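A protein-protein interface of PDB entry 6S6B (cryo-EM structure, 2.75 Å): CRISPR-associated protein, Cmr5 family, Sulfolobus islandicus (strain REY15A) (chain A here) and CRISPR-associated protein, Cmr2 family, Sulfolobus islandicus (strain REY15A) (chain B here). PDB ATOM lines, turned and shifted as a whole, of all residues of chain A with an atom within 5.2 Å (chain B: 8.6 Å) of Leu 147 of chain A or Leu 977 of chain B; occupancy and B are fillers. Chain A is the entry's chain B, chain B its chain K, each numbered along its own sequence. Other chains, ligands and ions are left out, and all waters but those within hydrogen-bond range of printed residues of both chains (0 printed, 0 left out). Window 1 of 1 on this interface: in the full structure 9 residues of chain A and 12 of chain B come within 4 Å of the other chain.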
ATOM      1  N   ALA A  10     -33.539 -17.678  16.141  1.00  0.00           N
ATOM      2  CA  ALA A  10     -32.777 -16.521  16.587  1.00  0.00           C
ATOM      3  C   ALA A  10     -31.398 -16.899  17.096  1.00  0.00           C
ATOM      4  O   ALA A  10     -30.506 -16.050  17.117  1.00  0.00           O
ATOM      5  CB  ALA A  10     -33.540 -15.777  17.678  1.00  0.00           C
ATOM      6  N   LEU A  11     -31.197 -18.149  17.502  1.00  0.00           N
ATOM      7  CA  LEU A  11     -29.899 -18.553  18.018  1.00  0.00           C
ATOM      8  C   LEU A  11     -28.939 -18.976  16.917  1.00  0.00           C
ATOM      9  O   LEU A  11     -27.730 -18.765  17.049  1.00  0.00           O
ATOM     10  CB  LEU A  11     -30.072 -19.683  19.024  1.00  0.00           C
ATOM     11  CG  LEU A  11     -30.515 -19.217  20.401  1.00  0.00           C
ATOM     12  CD1 LEU A  11     -31.098 -20.366  21.173  1.00  0.00           C
ATOM     13  CD2 LEU A  11     -29.325 -18.642  21.128  1.00  0.00           C
ATOM     14  N   PHE A  14     -28.149 -15.536  14.957  1.00  0.00           N
ATOM     15  CA  PHE A  14     -27.247 -14.686  15.721  1.00  0.00           C
ATOM     16  C   PHE A  14     -25.830 -15.241  15.710  1.00  0.00           C
ATOM     17  O   PHE A  14     -24.865 -14.504  15.486  1.00  0.00           O
ATOM     18  CB  PHE A  14     -27.756 -14.533  17.151  1.00  0.00           C
ATOM     19  CG  PHE A  14     -26.860 -13.716  18.024  1.00  0.00           C
ATOM     20  CD1 PHE A  14     -26.923 -12.340  18.001  1.00  0.00           C
ATOM     21  CD2 PHE A  14     -25.952 -14.322  18.863  1.00  0.00           C
ATOM     22  CE1 PHE A  14     -26.096 -11.589  18.798  1.00  0.00           C
ATOM     23  CE2 PHE A  14     -25.125 -13.575  19.659  1.00  0.00           C
ATOM     24  CZ  PHE A  14     -25.198 -12.207  19.628  1.00  0.00           C
ATOM     25  N   ALA A 143     -36.092 -11.424  20.147  1.00  0.00           N
ATOM     26  CA  ALA A 143     -35.096 -12.334  20.693  1.00  0.00           C
ATOM     27  C   ALA A 143     -33.695 -11.931  20.264  1.00  0.00           C
ATOM     28  O   ALA A 143     -32.754 -11.996  21.062  1.00  0.00           O
ATOM     29  CB  ALA A 143     -35.398 -13.764  20.259  1.00  0.00           C
ATOM     30  N   ILE A 144     -33.536 -11.519  19.005  1.00  0.00           N
ATOM     31  CA  ILE A 144     -32.242 -11.039  18.533  1.00  0.00           C
ATOM     32  C   ILE A 144     -31.804  -9.827  19.338  1.00  0.00           C
ATOM     33  O   ILE A 144     -30.623  -9.672  19.666  1.00  0.00           O
ATOM     34  CB  ILE A 144     -32.308 -10.719  17.029  1.00  0.00           C
ATOM     35  CG1 ILE A 144     -32.600 -11.982  16.223  1.00  0.00           C
ATOM     36  CG2 ILE A 144     -31.018 -10.074  16.569  1.00  0.00           C
ATOM     37  CD1 ILE A 144     -31.425 -12.904  16.091  1.00  0.00           C
ATOM     38  N   LYS A 145     -32.749  -8.948  19.669  1.00  0.00           N
ATOM     39  CA  LYS A 145     -32.434  -7.802  20.509  1.00  0.00           C
ATOM     40  C   LYS A 145     -31.906  -8.239  21.866  1.00  0.00           C
ATOM     41  O   LYS A 145     -30.938  -7.669  22.376  1.00  0.00           O
ATOM     42  CB  LYS A 145     -33.670  -6.925  20.674  1.00  0.00           C
ATOM     43  CG  LYS A 145     -33.569  -5.924  21.794  1.00  0.00           C
ATOM     44  CD  LYS A 145     -34.786  -5.029  21.824  1.00  0.00           C
ATOM     45  CE  LYS A 145     -34.699  -4.021  22.947  1.00  0.00           C
ATOM     46  NZ  LYS A 145     -35.485  -2.804  22.630  1.00  0.00           N
ATOM     47  N   ARG A 146     -32.524  -9.255  22.464  1.00  0.00           N
ATOM     48  CA  ARG A 146     -32.092  -9.700  23.781  1.00  0.00           C
ATOM     49  C   ARG A 146     -30.743 -10.396  23.718  1.00  0.00           C
ATOM     50  O   ARG A 146     -29.908 -10.224  24.611  1.00  0.00           O
ATOM     51  CB  ARG A 146     -33.137 -10.627  24.385  1.00  0.00           C
ATOM     52  CG  ARG A 146     -32.895 -10.954  25.841  1.00  0.00           C
ATOM     53  CD  ARG A 146     -34.141 -11.514  26.482  1.00  0.00           C
ATOM     54  NE  ARG A 146     -35.346 -11.048  25.810  1.00  0.00           N
ATOM     55  CZ  ARG A 146     -35.914  -9.868  26.025  1.00  0.00           C
ATOM     56  NH1 ARG A 146     -35.387  -9.024  26.899  1.00  0.00           N
ATOM     57  NH2 ARG A 146     -37.007  -9.534  25.360  1.00  0.00           N
ATOM     58  N   LEU A 147     -30.515 -11.198  22.678  1.00  0.00           N
ATOM     59  CA  LEU A 147     -29.238 -11.890  22.548  1.00  0.00           C
ATOM     60  C   LEU A 147     -28.096 -10.905  22.353  1.00  0.00           C
ATOM     61  O   LEU A 147     -26.988 -11.118  22.858  1.00  0.00           O
ATOM     62  CB  LEU A 147     -29.298 -12.868  21.382  1.00  0.00           C
ATOM     63  CG  LEU A 147     -29.974 -14.197  21.670  1.00  0.00           C
ATOM     64  CD1 LEU A 147     -30.438 -14.815  20.377  1.00  0.00           C
ATOM     65  CD2 LEU A 147     -29.011 -15.108  22.385  1.00  0.00           C
ATOM     66  N   SER A 148     -28.345  -9.830  21.610  1.00  0.00           N
ATOM     67  CA  SER A 148     -27.324  -8.816  21.390  1.00  0.00           C
ATOM     68  C   SER A 148     -26.888  -8.191  22.704  1.00  0.00           C
ATOM     69  O   SER A 148     -25.699  -8.162  23.033  1.00  0.00           O
ATOM     70  CB  SER A 148     -27.858  -7.751  20.440  1.00  0.00           C
ATOM     71  OG  SER A 148     -28.190  -8.327  19.197  1.00  0.00           O
ATOM     72  N   GLU A 149     -27.851  -7.680  23.471  1.00  0.00           N
ATOM     73  CA  GLU A 149     -27.536  -7.033  24.737  1.00  0.00           C
ATOM     74  C   GLU A 149     -26.820  -7.975  25.694  1.00  0.00           C
ATOM     75  O   GLU A 149     -26.090  -7.520  26.579  1.00  0.00           O
ATOM     76  CB  GLU A 149     -28.814  -6.504  25.376  1.00  0.00           C
ATOM     77  CG  GLU A 149     -29.650  -5.639  24.456  1.00  0.00           C
ATOM     78  CD  GLU A 149     -30.981  -5.250  25.070  1.00  0.00           C
ATOM     79  OE1 GLU A 149     -31.525  -6.039  25.867  1.00  0.00           O
ATOM     80  OE2 GLU A 149     -31.485  -4.152  24.761  1.00  0.00           O
ATOM     81  N   ALA A 150     -27.009  -9.281  25.533  1.00  0.00           N
ATOM     82  CA  ALA A 150     -26.407 -10.249  26.436  1.00  0.00           C
ATOM     83  C   ALA A 150     -25.044 -10.724  25.949  1.00  0.00           C
ATOM     84  O   ALA A 150     -24.081 -10.746  26.721  1.00  0.00           O
ATOM     85  CB  ALA A 150     -27.343 -11.443  26.619  1.00  0.00           C
ATOM     86  N   LEU A 151     -24.943 -11.106  24.678  1.00  0.00           N
ATOM     87  CA  LEU A 151     -23.727 -11.731  24.174  1.00  0.00           C
ATOM     88  C   LEU A 151     -22.701 -10.717  23.696  1.00  0.00           C
ATOM     89  O   LEU A 151     -21.499 -10.930  23.872  1.00  0.00           O
ATOM     90  CB  LEU A 151     -24.057 -12.695  23.034  1.00  0.00           C
ATOM     91  CG  LEU A 151     -24.549 -14.098  23.396  1.00  0.00           C
ATOM     92  CD1 LEU A 151     -23.522 -14.819  24.244  1.00  0.00           C
ATOM     93  CD2 LEU A 151     -25.901 -14.079  24.080  1.00  0.00           C
ATOM     94  N   ILE A 152     -23.142  -9.624  23.083  1.00  0.00           N
ATOM     95  CA  ILE A 152     -22.227  -8.600  22.594  1.00  0.00           C
ATOM     96  C   ILE A 152     -21.865  -7.698  23.767  1.00  0.00           C
ATOM     97  O   ILE A 152     -22.672  -6.876  24.205  1.00  0.00           O
ATOM     98  CB  ILE A 152     -22.837  -7.793  21.445  1.00  0.00           C
ATOM     99  CG1 ILE A 152     -23.121  -8.697  20.252  1.00  0.00           C
ATOM    100  CG2 ILE A 152     -21.902  -6.678  21.043  1.00  0.00           C
ATOM    101  CD1 ILE A 152     -23.776  -7.986  19.111  1.00  0.00           C
ATOM    102  N   TYR B 965     -36.508 -14.314  29.366  1.00  0.00           N
ATOM    103  CA  TYR B 965     -35.214 -14.943  29.167  1.00  0.00           C
ATOM    104  C   TYR B 965     -35.307 -16.455  29.085  1.00  0.00           C
ATOM    105  O   TYR B 965     -34.351 -17.090  28.637  1.00  0.00           O
ATOM    106  CB  TYR B 965     -34.260 -14.566  30.296  1.00  0.00           C
ATOM    107  CG  TYR B 965     -33.881 -13.113  30.319  1.00  0.00           C
ATOM    108  CD1 TYR B 965     -34.755 -12.160  30.811  1.00  0.00           C
ATOM    109  CD2 TYR B 965     -32.652 -12.693  29.850  1.00  0.00           C
ATOM    110  CE1 TYR B 965     -34.416 -10.835  30.835  1.00  0.00           C
ATOM    111  CE2 TYR B 965     -32.304 -11.369  29.873  1.00  0.00           C
ATOM    112  CZ  TYR B 965     -33.191 -10.445  30.366  1.00  0.00           C
ATOM    113  OH  TYR B 965     -32.851  -9.116  30.389  1.00  0.00           O
ATOM    114  N   LEU B 968     -35.075 -18.381  25.534  1.00  0.00           N
ATOM    115  CA  LEU B 968     -33.730 -18.405  24.978  1.00  0.00           C
ATOM    116  C   LEU B 968     -32.831 -19.353  25.754  1.00  0.00           C
ATOM    117  O   LEU B 968     -32.061 -20.110  25.158  1.00  0.00           O
ATOM    118  CB  LEU B 968     -33.134 -17.001  24.971  1.00  0.00           C
ATOM    119  CG  LEU B 968     -33.591 -16.040  23.881  1.00  0.00           C
ATOM    120  CD1 LEU B 968     -33.122 -14.647  24.217  1.00  0.00           C
ATOM    121  CD2 LEU B 968     -33.058 -16.470  22.538  1.00  0.00           C
ATOM    122  N   ILE B 969     -32.908 -19.324  27.085  1.00  0.00           N
ATOM    123  CA  ILE B 969     -32.081 -20.221  27.883  1.00  0.00           C
ATOM    124  C   ILE B 969     -32.487 -21.667  27.651  1.00  0.00           C
ATOM    125  O   ILE B 969     -31.664 -22.580  27.777  1.00  0.00           O
ATOM    126  CB  ILE B 969     -32.162 -19.842  29.370  1.00  0.00           C
ATOM    127  CG1 ILE B 969     -31.739 -18.392  29.571  1.00  0.00           C
ATOM    128  CG2 ILE B 969     -31.262 -20.734  30.194  1.00  0.00           C
ATOM    129  CD1 ILE B 969     -32.095 -17.849  30.924  1.00  0.00           C
ATOM    130  N   VAL B 970     -33.748 -21.904  27.303  1.00  0.00           N
ATOM    131  CA  VAL B 970     -34.183 -23.255  26.971  1.00  0.00           C
ATOM    132  C   VAL B 970     -33.601 -23.679  25.630  1.00  0.00           C
ATOM    133  O   VAL B 970     -32.897 -24.689  25.528  1.00  0.00           O
ATOM    134  CB  VAL B 970     -35.718 -23.344  26.969  1.00  0.00           C
ATOM    135  CG1 VAL B 970     -36.173 -24.575  26.215  1.00  0.00           C
ATOM    136  CG2 VAL B 970     -36.244 -23.364  28.390  1.00  0.00           C
ATOM    137  N   ALA B 971     -33.877 -22.901  24.584  1.00  0.00           N
ATOM    138  CA  ALA B 971     -33.481 -23.287  23.236  1.00  0.00           C
ATOM    139  C   ALA B 971     -31.974 -23.279  23.039  1.00  0.00           C
ATOM    140  O   ALA B 971     -31.485 -23.901  22.092  1.00  0.00           O
ATOM    141  CB  ALA B 971     -34.142 -22.364  22.216  1.00  0.00           C
ATOM    142  N   SER B 972     -31.228 -22.600  23.902  1.00  0.00           N
ATOM    143  CA  SER B 972     -29.786 -22.496  23.733  1.00  0.00           C
ATOM    144  C   SER B 972     -29.112 -23.741  24.286  1.00  0.00           C
ATOM    145  O   SER B 972     -29.262 -24.064  25.468  1.00  0.00           O
ATOM    146  CB  SER B 972     -29.254 -21.247  24.426  1.00  0.00           C
ATOM    147  OG  SER B 972     -27.848 -21.174  24.309  1.00  0.00           O
ATOM    148  N   ASP B 973     -28.362 -24.433  23.433  1.00  0.00           N
ATOM    149  CA  ASP B 973     -27.676 -25.658  23.814  1.00  0.00           C
ATOM    150  C   ASP B 973     -26.169 -25.476  23.908  1.00  0.00           C
ATOM    151  O   ASP B 973     -25.446 -26.461  24.086  1.00  0.00           O
ATOM    152  CB  ASP B 973     -28.015 -26.775  22.828  1.00  0.00           C
ATOM    153  CG  ASP B 973     -27.880 -26.339  21.383  1.00  0.00           C
ATOM    154  OD1 ASP B 973     -27.145 -25.366  21.115  1.00  0.00           O
ATOM    155  OD2 ASP B 973     -28.512 -26.971  20.512  1.00  0.00           O
ATOM    156  N   GLU B 974     -25.677 -24.249  23.792  1.00  0.00           N
ATOM    157  CA  GLU B 974     -24.253 -23.957  23.895  1.00  0.00           C
ATOM    158  C   GLU B 974     -24.029 -23.232  25.214  1.00  0.00           C
ATOM    159  O   GLU B 974     -24.461 -22.087  25.380  1.00  0.00           O
ATOM    160  CB  GLU B 974     -23.779 -23.134  22.701  1.00  0.00           C
ATOM    161  CG  GLU B 974     -24.183 -23.749  21.373  1.00  0.00           C
ATOM    162  CD  GLU B 974     -23.283 -23.339  20.227  1.00  0.00           C
ATOM    163  OE1 GLU B 974     -23.636 -23.617  19.062  1.00  0.00           O
ATOM    164  OE2 GLU B 974     -22.214 -22.755  20.492  1.00  0.00           O
ATOM    165  N   LYS B 975     -23.351 -23.903  26.144  1.00  0.00           N
ATOM    166  CA  LYS B 975     -23.330 -23.447  27.528  1.00  0.00           C
ATOM    167  C   LYS B 975     -22.592 -22.128  27.692  1.00  0.00           C
ATOM    168  O   LYS B 975     -22.869 -21.385  28.638  1.00  0.00           O
ATOM    169  CB  LYS B 975     -22.709 -24.520  28.417  1.00  0.00           C
ATOM    170  CG  LYS B 975     -23.616 -25.721  28.638  1.00  0.00           C
ATOM    171  CD  LYS B 975     -22.860 -26.899  29.235  1.00  0.00           C
ATOM    172  CE  LYS B 975     -21.553 -27.155  28.496  1.00  0.00           C
ATOM    173  NZ  LYS B 975     -21.735 -27.267  27.021  1.00  0.00           N
ATOM    174  N   TYR B 976     -21.654 -21.815  26.799  1.00  0.00           N
ATOM    175  CA  TYR B 976     -21.009 -20.509  26.860  1.00  0.00           C
ATOM    176  C   TYR B 976     -21.991 -19.384  26.577  1.00  0.00           C
ATOM    177  O   TYR B 976     -21.743 -18.244  26.975  1.00  0.00           O
ATOM    178  CB  TYR B 976     -19.852 -20.436  25.865  1.00  0.00           C
ATOM    179  CG  TYR B 976     -20.294 -20.046  24.476  1.00  0.00           C
ATOM    180  CD1 TYR B 976     -20.920 -20.962  23.649  1.00  0.00           C
ATOM    181  CD2 TYR B 976     -20.087 -18.761  23.990  1.00  0.00           C
ATOM    182  CE1 TYR B 976     -21.332 -20.611  22.379  1.00  0.00           C
ATOM    183  CE2 TYR B 976     -20.494 -18.403  22.720  1.00  0.00           C
ATOM    184  CZ  TYR B 976     -21.116 -19.336  21.920  1.00  0.00           C
ATOM    185  OH  TYR B 976     -21.528 -19.000  20.650  1.00  0.00           O
ATOM    186  N   LEU B 977     -23.093 -19.683  25.895  1.00  0.00           N
ATOM    187  CA  LEU B 977     -24.094 -18.680  25.570  1.00  0.00           C
ATOM    188  C   LEU B 977     -25.131 -18.538  26.674  1.00  0.00           C
ATOM    189  O   LEU B 977     -25.620 -17.432  26.926  1.00  0.00           O
ATOM    190  CB  LEU B 977     -24.764 -19.035  24.240  1.00  0.00           C
ATOM    191  CG  LEU B 977     -25.622 -17.990  23.531  1.00  0.00           C
ATOM    192  CD1 LEU B 977     -25.558 -18.215  22.033  1.00  0.00           C
ATOM    193  CD2 LEU B 977     -27.060 -18.046  23.998  1.00  0.00           C
ATOM    194  N   THR B 978     -25.476 -19.635  27.348  1.00  0.00           N
ATOM    195  CA  THR B 978     -26.428 -19.542  28.444  1.00  0.00           C
ATOM    196  C   THR B 978     -25.808 -18.899  29.675  1.00  0.00           C
ATOM    197  O   THR B 978     -26.492 -18.168  30.397  1.00  0.00           O
ATOM    198  CB  THR B 978     -26.967 -20.920  28.793  1.00  0.00           C
ATOM    199  OG1 THR B 978     -25.879 -21.767  29.173  1.00  0.00           O
ATOM    200  CG2 THR B 978     -27.664 -21.519  27.605  1.00  0.00           C
ATOM    201  N   GLU B 979     -24.523 -19.147  29.929  1.00  0.00           N
ATOM    202  CA  GLU B 979     -23.871 -18.502  31.060  1.00  0.00           C
ATOM    203  C   GLU B 979     -23.780 -16.997  30.890  1.00  0.00           C
ATOM    204  O   GLU B 979     -23.339 -16.310  31.817  1.00  0.00           O
ATOM    205  CB  GLU B 979     -22.476 -19.080  31.274  1.00  0.00           C
ATOM    206  CG  GLU B 979     -21.527 -18.857  30.112  1.00  0.00           C
ATOM    207  CD  GLU B 979     -20.115 -19.330  30.405  1.00  0.00           C
ATOM    208  OE1 GLU B 979     -19.864 -19.795  31.537  1.00  0.00           O
ATOM    209  OE2 GLU B 979     -19.257 -19.239  29.503  1.00  0.00           O
ATOM    210  N   PHE B 980     -24.177 -16.472  29.735  1.00  0.00           N
ATOM    211  CA  PHE B 980     -24.298 -15.038  29.522  1.00  0.00           C
ATOM    212  C   PHE B 980     -25.736 -14.560  29.566  1.00  0.00           C
ATOM    213  O   PHE B 980     -25.979 -13.395  29.886  1.00  0.00           O
ATOM    214  CB  PHE B 980     -23.689 -14.646  28.175  1.00  0.00           C
ATOM    215  CG  PHE B 980     -22.197 -14.542  28.194  1.00  0.00           C
ATOM    216  CD1 PHE B 980     -21.535 -14.136  29.334  1.00  0.00           C
ATOM    217  CD2 PHE B 980     -21.456 -14.850  27.073  1.00  0.00           C
ATOM    218  CE1 PHE B 980     -20.167 -14.039  29.354  1.00  0.00           C
ATOM    219  CE2 PHE B 980     -20.087 -14.754  27.088  1.00  0.00           C
ATOM    220  CZ  PHE B 980     -19.442 -14.347  28.231  1.00  0.00           C
ATOM    221  N   LEU B 981     -26.692 -15.430  29.242  1.00  0.00           N
ATOM    222  CA  LEU B 981     -28.095 -15.042  29.306  1.00  0.00           C
ATOM    223  C   LEU B 981     -28.571 -14.942  30.747  1.00  0.00           C
ATOM    224  O   LEU B 981     -29.355 -14.051  31.085  1.00  0.00           O
ATOM    225  CB  LEU B 981     -28.947 -16.035  28.526  1.00  0.00           C
ATOM    226  CG  LEU B 981     -28.949 -15.837  27.013  1.00  0.00           C
ATOM    227  CD1 LEU B 981     -29.651 -16.986  26.328  1.00  0.00           C
ATOM    228  CD2 LEU B 981     -29.614 -14.524  26.662  1.00  0.00           C
ATOM    229  N   VAL B 982     -28.109 -15.843  31.613  1.00  0.00           N
ATOM    230  CA  VAL B 982     -28.471 -15.727  33.017  1.00  0.00           C
ATOM    231  C   VAL B 982     -27.647 -14.644  33.689  1.00  0.00           C
ATOM    232  O   VAL B 982     -28.116 -14.003  34.632  1.00  0.00           O
ATOM    233  CB  VAL B 982     -28.321 -17.077  33.735  1.00  0.00           C
ATOM    234  CG1 VAL B 982     -29.031 -18.161  32.958  1.00  0.00           C
ATOM    235  CG2 VAL B 982     -26.867 -17.423  33.927  1.00  0.00           C
ATOM    236  N   LYS B 983     -26.420 -14.416  33.223  1.00  0.00           N
ATOM    237  CA  LYS B 983     -25.649 -13.283  33.713  1.00  0.00           C
ATOM    238  C   LYS B 983     -26.316 -11.972  33.334  1.00  0.00           C
ATOM    239  O   LYS B 983     -26.228 -10.990  34.076  1.00  0.00           O
ATOM    240  CB  LYS B 983     -24.226 -13.352  33.160  1.00  0.00           C
ATOM    241  CG  LYS B 983     -23.260 -12.357  33.768  1.00  0.00           C
ATOM    242  CD  LYS B 983     -23.101 -11.128  32.894  1.00  0.00           C
ATOM    243  CE  LYS B 983     -22.223 -10.086  33.564  1.00  0.00           C
ATOM    244  NZ  LYS B 983     -22.196  -8.800  32.811  1.00  0.00           N
ATOM    245  N   ASP B 984     -26.998 -11.944  32.192  1.00  0.00           N
ATOM    246  CA  ASP B 984     -27.718 -10.752  31.767  1.00  0.00           C
ATOM    247  C   ASP B 984     -29.032 -10.618  32.517  1.00  0.00           C
ATOM    248  O   ASP B 984     -29.365  -9.539  33.013  1.00  0.00           O
ATOM    249  CB  ASP B 984     -27.967 -10.808  30.261  1.00  0.00           C
ATOM    250  CG  ASP B 984     -28.765  -9.628  29.756  1.00  0.00           C
ATOM    251  OD1 ASP B 984     -28.639  -8.531  30.331  1.00  0.00           O
ATOM    252  OD2 ASP B 984     -29.519  -9.796  28.775  1.00  0.00           O
ATOM    253  N   ARG B 988     -29.734  -7.298  34.809  1.00  0.00           N
ATOM    254  CA  ARG B 988     -30.738  -6.350  34.348  1.00  0.00           C
ATOM    255  C   ARG B 988     -31.578  -5.858  35.511  1.00  0.00           C
ATOM    256  O   ARG B 988     -31.533  -4.681  35.881  1.00  0.00           O
ATOM    257  CB  ARG B 988     -31.622  -6.996  33.289  1.00  0.00           C
ATOM    258  CG  ARG B 988     -30.982  -7.052  31.940  1.00  0.00           C
ATOM    259  CD  ARG B 988     -30.236  -5.771  31.653  1.00  0.00           C
ATOM    260  NE  ARG B 988     -29.859  -5.681  30.251  1.00  0.00           N
ATOM    261  CZ  ARG B 988     -30.706  -5.392  29.272  1.00  0.00           C
ATOM    262  NH1 ARG B 988     -31.983  -5.159  29.539  1.00  0.00           N
ATOM    263  NH2 ARG B 988     -30.275  -5.332  28.024  1.00  0.00           N
ATOM    264  N   GLU B1001     -23.673 -23.902  36.363  1.00  0.00           N
ATOM    265  CA  GLU B1001     -23.500 -24.150  34.938  1.00  0.00           C
ATOM    266  C   GLU B1001     -23.681 -25.629  34.594  1.00  0.00           C
ATOM    267  O   GLU B1001     -23.805 -25.960  33.416  1.00  0.00           O
ATOM    268  CB  GLU B1001     -22.136 -23.642  34.418  1.00  0.00           C
ATOM    269  CG  GLU B1001     -21.885 -23.629  32.923  1.00  0.00           C
ATOM    270  CD  GLU B1001     -21.325 -24.940  32.415  1.00  0.00           C
ATOM    271  OE1 GLU B1001     -21.204 -25.099  31.185  1.00  0.00           O
ATOM    272  OE2 GLU B1001     -21.002 -25.809  33.249  1.00  0.00           O
ATOM    273  N   TYR B1004     -27.855 -26.178  33.391  1.00  0.00           N
ATOM    274  CA  TYR B1004     -28.399 -25.661  32.141  1.00  0.00           C
ATOM    275  C   TYR B1004     -28.975 -26.833  31.362  1.00  0.00           C
ATOM    276  O   TYR B1004     -28.255 -27.543  30.656  1.00  0.00           O
ATOM    277  CB  TYR B1004     -27.325 -24.919  31.356  1.00  0.00           C
ATOM    278  CG  TYR B1004     -26.852 -23.670  32.056  1.00  0.00           C
ATOM    279  CD1 TYR B1004     -27.730 -22.897  32.802  1.00  0.00           C
ATOM    280  CD2 TYR B1004     -25.531 -23.267  31.979  1.00  0.00           C
ATOM    281  CE1 TYR B1004     -27.304 -21.761  33.446  1.00  0.00           C
ATOM    282  CE2 TYR B1004     -25.099 -22.131  32.616  1.00  0.00           C
ATOM    283  CZ  TYR B1004     -25.987 -21.384  33.349  1.00  0.00           C
ATOM    284  OH  TYR B1004     -25.548 -20.251  33.985  1.00  0.00           O
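Hydrophobic or aromatic side chains of chain B that line the printed part of chain A: Tyr 965, Leu 968, Ala 971, Leu 977, Phe 980 and Leu 981. Of the 13 printed residues of chain A, 6 touch a printed residue of chain B. Among the printed residues, Asp or Glu carboxylates within 4 Å of a Lys or Arg side-chain nitrogen of the other chain: Glu 149 of chain A with Arg 988 of chain B (2.6 Å).
Among the printed residues, merely in contact across the chains: Ala 150 of chain A with Asp 984 of chain B (3.5 Å), Leu 151 of chain A with Phe 980 of chain B (3.5 Å), Leu 11 of chain A with Ser 972 of chain B (3.5 Å), Leu 11 of chain A with Ala 971 of chain B (3.6 Å), Leu 11 of chain A with Leu 977 of chain B (3.7 Å), Leu 147 of chain A with Leu 968 of chain B (3.8 Å), Ala 150 of chain A with Leu 981 of chain B (3.8 Å), Arg 146 of chain A with Tyr 965 of chain B (3.9 Å), Leu 151 of chain A with Leu 977 of chain B (3.9 Å), Leu 147 of chain A with Leu 977 of chain B (3.9 Å) and Arg 146 of chain A with Leu 968 of chain B (3.998 Å).
OE1 of Glu 149 of chain A is in salt-bridge range of NH2 of Arg 988 of chain B, at 2.6 Å.
Leu 147 of chain A touches just these residues of chain B: Leu 968 (3.8 Å) and Leu 977 (3.9 Å). Leu 977 of chain B touches just these residues of chain A: Leu 11 (3.7 Å), Leu 147 (3.9 Å) and Leu 151 (3.9 Å). No residue of chain B comes within 4 Å of Ser 148 of chain A. Printed residues of chain A within 4 Å of Arg 988 of chain B: Glu 149. Printed residues of chain B within 4 Å of Arg 146 of chain A: Tyr 965 and Leu 968. Val 970 of chain B touches none of the printed residues of chain A. The nearest residue of chain B that does not touch Leu 147 of chain A is Leu 981 of chain B (4.4 Å).
OD1 of Asp 984 of chain B is in salt-bridge range of NE of Arg 988 of chain B.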
